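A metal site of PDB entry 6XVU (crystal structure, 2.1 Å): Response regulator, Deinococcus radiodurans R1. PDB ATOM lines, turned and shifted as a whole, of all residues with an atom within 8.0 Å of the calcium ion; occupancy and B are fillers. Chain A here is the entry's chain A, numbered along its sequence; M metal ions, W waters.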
ATOM      1  N   VAL A  28      15.925  -0.789 -29.138  1.00  0.00           N
ATOM      2  CA  VAL A  28      16.170  -1.201 -27.722  1.00  0.00           C
ATOM      3  C   VAL A  28      15.614  -2.601 -27.574  1.00  0.00           C
ATOM      4  O   VAL A  28      14.402  -2.787 -27.646  1.00  0.00           O
ATOM      5  CB  VAL A  28      15.575  -0.244 -26.685  1.00  0.00           C
ATOM      6  CG1 VAL A  28      16.132  -0.488 -25.291  1.00  0.00           C
ATOM      7  CG2 VAL A  28      15.768   1.224 -27.079  1.00  0.00           C
ATOM      8  N   GLU A  29      16.499  -3.560 -27.490  1.00  0.00           N
ATOM      9  CA  GLU A  29      16.178  -5.002 -27.591  1.00  0.00           C
ATOM     10  C   GLU A  29      17.283  -5.783 -26.905  1.00  0.00           C
ATOM     11  O   GLU A  29      18.461  -5.448 -27.148  1.00  0.00           O
ATOM     12  CB  GLU A  29      16.044  -5.346 -29.069  1.00  0.00           C
ATOM     13  CG  GLU A  29      15.924  -6.840 -29.339  1.00  0.00           C
ATOM     14  CD  GLU A  29      14.692  -7.475 -28.732  1.00  0.00           C
ATOM     15  OE1 GLU A  29      13.577  -7.159 -29.199  1.00  0.00           O
ATOM     16  OE2 GLU A  29      14.860  -8.305 -27.782  1.00  0.00           O
ATOM     17  N   ASP A  30      16.928  -6.734 -26.038  1.00  0.00           N
ATOM     18  CA  ASP A  30      17.878  -7.552 -25.266  1.00  0.00           C
ATOM     19  C   ASP A  30      18.303  -8.804 -26.060  1.00  0.00           C
ATOM     20  O   ASP A  30      19.419  -9.234 -25.894  1.00  0.00           O
ATOM     21  CB  ASP A  30      17.293  -7.897 -23.898  1.00  0.00           C
ATOM     22  CG  ASP A  30      15.948  -8.629 -23.927  1.00  0.00           C
ATOM     23  OD1 ASP A  30      15.139  -8.324 -24.794  1.00  0.00           O
ATOM     24  OD2 ASP A  30      15.738  -9.546 -23.091  1.00  0.00           O
ATOM     25  N   ASN A  31      17.438  -9.334 -26.929  1.00  0.00           N
ATOM     26  CA  ASN A  31      17.711 -10.592 -27.650  1.00  0.00           C
ATOM     27  C   ASN A  31      18.452 -10.313 -28.979  1.00  0.00           C
ATOM     28  O   ASN A  31      17.931  -9.610 -29.876  1.00  0.00           O
ATOM     29  CB  ASN A  31      16.433 -11.414 -27.808  1.00  0.00           C
ATOM     30  CG  ASN A  31      16.821 -12.818 -28.250  1.00  0.00           C
ATOM     31  OD1 ASN A  31      17.671 -13.477 -27.631  1.00  0.00           O
ATOM     32  ND2 ASN A  31      16.238 -13.260 -29.345  1.00  0.00           N
ATOM     33  N   ASP A  34      16.695 -10.926 -32.374  1.00  0.00           N
ATOM     34  CA  ASP A  34      15.727  -9.864 -32.770  1.00  0.00           C
ATOM     35  C   ASP A  34      16.503  -8.698 -33.415  1.00  0.00           C
ATOM     36  O   ASP A  34      16.010  -8.076 -34.369  1.00  0.00           O
ATOM     37  CB  ASP A  34      14.882  -9.455 -31.575  1.00  0.00           C
ATOM     38  CG  ASP A  34      13.904 -10.504 -31.038  1.00  0.00           C
ATOM     39  OD1 ASP A  34      14.321 -11.400 -30.263  1.00  0.00           O
ATOM     40  OD2 ASP A  34      12.727 -10.425 -31.377  1.00  0.00           O
ATOM     41  N   ARG A  55      20.803  -2.467 -25.557  1.00  0.00           N
ATOM     42  CA  ARG A  55      20.386  -3.825 -25.089  1.00  0.00           C
ATOM     43  C   ARG A  55      19.371  -3.737 -23.947  1.00  0.00           C
ATOM     44  O   ARG A  55      18.797  -4.754 -23.611  1.00  0.00           O
ATOM     45  CB  ARG A  55      21.608  -4.620 -24.649  1.00  0.00           C
ATOM     46  CG  ARG A  55      22.574  -4.979 -25.784  1.00  0.00           C
ATOM     47  CD  ARG A  55      21.982  -5.375 -27.130  1.00  0.00           C
ATOM     48  NE  ARG A  55      21.559  -6.775 -27.060  1.00  0.00           N
ATOM     49  CZ  ARG A  55      22.363  -7.847 -27.247  1.00  0.00           C
ATOM     50  NH1 ARG A  55      23.640  -7.725 -27.563  1.00  0.00           N
ATOM     51  NH2 ARG A  55      21.893  -9.061 -27.097  1.00  0.00           N
ATOM     52  N   ASP A  80      11.379  -2.884 -26.966  1.00  0.00           N
ATOM     53  CA  ASP A  80      10.720  -4.085 -26.417  1.00  0.00           C
ATOM     54  C   ASP A  80      10.254  -3.783 -24.988  1.00  0.00           C
ATOM     55  O   ASP A  80      10.698  -2.765 -24.434  1.00  0.00           O
ATOM     56  CB  ASP A  80      11.721  -5.208 -26.586  1.00  0.00           C
ATOM     57  CG  ASP A  80      11.228  -6.539 -26.108  1.00  0.00           C
ATOM     58  OD1 ASP A  80      10.079  -6.923 -26.488  1.00  0.00           O
ATOM     59  OD2 ASP A  80      11.924  -7.032 -25.213  1.00  0.00           O
ATOM     60  N   LEU A  81       9.316  -4.534 -24.472  1.00  0.00           N
ATOM     61  CA  LEU A  81       8.735  -4.295 -23.117  1.00  0.00           C
ATOM     62  C   LEU A  81       9.608  -5.002 -22.080  1.00  0.00           C
ATOM     63  O   LEU A  81      10.054  -4.362 -21.136  1.00  0.00           O
ATOM     64  CB  LEU A  81       7.291  -4.805 -23.080  1.00  0.00           C
ATOM     65  CG  LEU A  81       6.305  -3.978 -23.909  1.00  0.00           C
ATOM     66  CD1 LEU A  81       4.881  -4.450 -23.651  1.00  0.00           C
ATOM     67  CD2 LEU A  81       6.464  -2.478 -23.682  1.00  0.00           C
ATOM     68  N   ASN A  82       9.854  -6.288 -22.282  1.00  0.00           N
ATOM     69  CA  ASN A  82      10.514  -7.143 -21.276  1.00  0.00           C
ATOM     70  C   ASN A  82      12.021  -7.122 -21.542  1.00  0.00           C
ATOM     71  O   ASN A  82      12.462  -7.809 -22.485  1.00  0.00           O
ATOM     72  CB  ASN A  82       9.938  -8.552 -21.233  1.00  0.00           C
ATOM     73  CG  ASN A  82      10.519  -9.299 -20.062  1.00  0.00           C
ATOM     74  OD1 ASN A  82      11.130  -8.692 -19.191  1.00  0.00           O
ATOM     75  ND2 ASN A  82      10.376 -10.604 -20.053  1.00  0.00           N
ATOM     76  N   MET A  83      12.756  -6.316 -20.775  1.00  0.00           N
ATOM     77  CA  MET A  83      14.219  -6.107 -20.932  1.00  0.00           C
ATOM     78  C   MET A  83      14.791  -5.950 -19.551  1.00  0.00           C
ATOM     79  O   MET A  83      14.131  -5.391 -18.690  1.00  0.00           O
ATOM     80  CB  MET A  83      14.554  -4.833 -21.714  1.00  0.00           C
ATOM     81  CG  MET A  83      13.976  -4.812 -23.101  1.00  0.00           C
ATOM     82  SD  MET A  83      14.557  -3.365 -24.018  1.00  0.00           S
ATOM     83  CE  MET A  83      13.641  -2.072 -23.149  1.00  0.00           C
ATOM     84  N   PRO A  84      16.024  -6.421 -19.301  1.00  0.00           N
ATOM     85  CA  PRO A  84      16.580  -6.315 -17.969  1.00  0.00           C
ATOM     86  C   PRO A  84      16.907  -4.861 -17.586  1.00  0.00           C
ATOM     87  O   PRO A  84      17.088  -4.036 -18.440  1.00  0.00           O
ATOM     88  CB  PRO A  84      17.811  -7.254 -18.046  1.00  0.00           C
ATOM     89  CG  PRO A  84      18.225  -7.214 -19.480  1.00  0.00           C
ATOM     90  CD  PRO A  84      16.940  -7.035 -20.272  1.00  0.00           C
ATOM     91  N   LEU A 109       7.838  -2.372 -29.984  1.00  0.00           N
ATOM     92  CA  LEU A 109       7.847  -3.558 -30.862  1.00  0.00           C
ATOM     93  C   LEU A 109       8.161  -4.743 -29.976  1.00  0.00           C
ATOM     94  O   LEU A 109       9.301  -4.833 -29.486  1.00  0.00           O
ATOM     95  CB  LEU A 109       8.887  -3.361 -31.978  1.00  0.00           C
ATOM     96  CG  LEU A 109       9.155  -4.585 -32.849  1.00  0.00           C
ATOM     97  CD1 LEU A 109       7.946  -4.926 -33.661  1.00  0.00           C
ATOM     98  CD2 LEU A 109      10.377  -4.338 -33.714  1.00  0.00           C
ATOM     99  N   THR A 110       7.171  -5.612 -29.756  1.00  0.00           N
ATOM    100  CA  THR A 110       7.205  -6.599 -28.672  1.00  0.00           C
ATOM    101  C   THR A 110       6.379  -7.821 -29.059  1.00  0.00           C
ATOM    102  O   THR A 110       5.474  -7.699 -29.937  1.00  0.00           O
ATOM    103  CB  THR A 110       6.721  -5.872 -27.411  1.00  0.00           C
ATOM    104  OG1 THR A 110       7.350  -6.490 -26.276  1.00  0.00           O
ATOM    105  CG2 THR A 110       5.201  -5.691 -27.381  1.00  0.00           C
ATOM    106  N   THR A 111       6.614  -8.976 -28.429  1.00  0.00           N
ATOM    107  CA  THR A 111       5.859 -10.218 -28.819  1.00  0.00           C
ATOM    108  C   THR A 111       4.480 -10.244 -28.092  1.00  0.00           C
ATOM    109  O   THR A 111       3.536 -10.813 -28.646  1.00  0.00           O
ATOM    110  CB  THR A 111       6.617 -11.526 -28.566  1.00  0.00           C
ATOM    111  OG1 THR A 111       6.852 -11.522 -27.173  1.00  0.00           O
ATOM    112  CG2 THR A 111       7.923 -11.749 -29.304  1.00  0.00           C
ATOM    113  N   LYS A 132       5.378  -8.124 -32.686  1.00  0.00           N
ATOM    114  CA  LYS A 132       6.234  -9.019 -33.516  1.00  0.00           C
ATOM    115  C   LYS A 132       5.386 -10.145 -34.074  1.00  0.00           C
ATOM    116  O   LYS A 132       4.708 -10.850 -33.366  1.00  0.00           O
ATOM    117  CB  LYS A 132       7.396  -9.577 -32.686  1.00  0.00           C
ATOM    118  CG  LYS A 132       8.410  -8.507 -32.281  1.00  0.00           C
ATOM    119  CD  LYS A 132       9.465  -9.063 -31.348  1.00  0.00           C
ATOM    120  CE  LYS A 132      10.401  -8.026 -30.807  1.00  0.00           C
ATOM    121  NZ  LYS A 132      11.214  -8.566 -29.707  1.00  0.00           N
HETATM  122 CA    CA M   1      12.872  -8.980 -24.463  1.00  0.00          CA
HETATM  123  O   HOH W   1      13.080  -9.497 -26.624  1.00  0.00           O
HETATM  124  O   HOH W   2      13.475 -10.679 -22.769  1.00  0.00           O
HETATM  125  O   HOH W   3      10.942 -10.001 -24.394  1.00  0.00           O
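Glu 29 touches the calcium ion. Within 4 Å of the calcium ion: Glu 29, Asp 30, Asp 80 and Asn 82. The nearest printed residue that does not touch the calcium ion is Met 83 (4.5 Å).
The calcium ion is bound by water W3 (2.2 Å), water W1 (2.2 Å), the side-chain carboxylate of Asp 80 (2.3 Å), the backbone carbonyl oxygen of Asn 82 (2.3 Å), the side-chain carboxylate of Asp 30 (2.4 Å) and water W2 (2.5 Å).
The side-chain amino group (NZ) of Lys 132 is in salt-bridge range of the side-chain carboxylate (OD1) of Asp 80, at 3.8 Å. The side-chain carboxylate of Asp 80 sits at hydrogen-bond distance from the side-chain hydroxyl of Thr 110, 2.8 Å away. O of Val 28 lies within hydrogen-bond range of N of Asp 80 (3.1 Å). The backbone carbonyl oxygen (O) of Asp 30 sits at hydrogen-bond distance from the guanidinium group (NH2) of Arg 55, at 2.8 Å. OE2 of Glu 29 sits at hydrogen-bond distance from N of Asn 31, at 2.9 Å. The side-chain carboxylate (OE1) of Glu 29 lies within salt-bridge range of the side-chain amino group (NZ) of Lys 132, at 2.8 Å. The guanidinium group (NE) of Arg 55 sits close to the backbone carbonyl oxygen (O) of Glu 29, 3.4 Å away.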
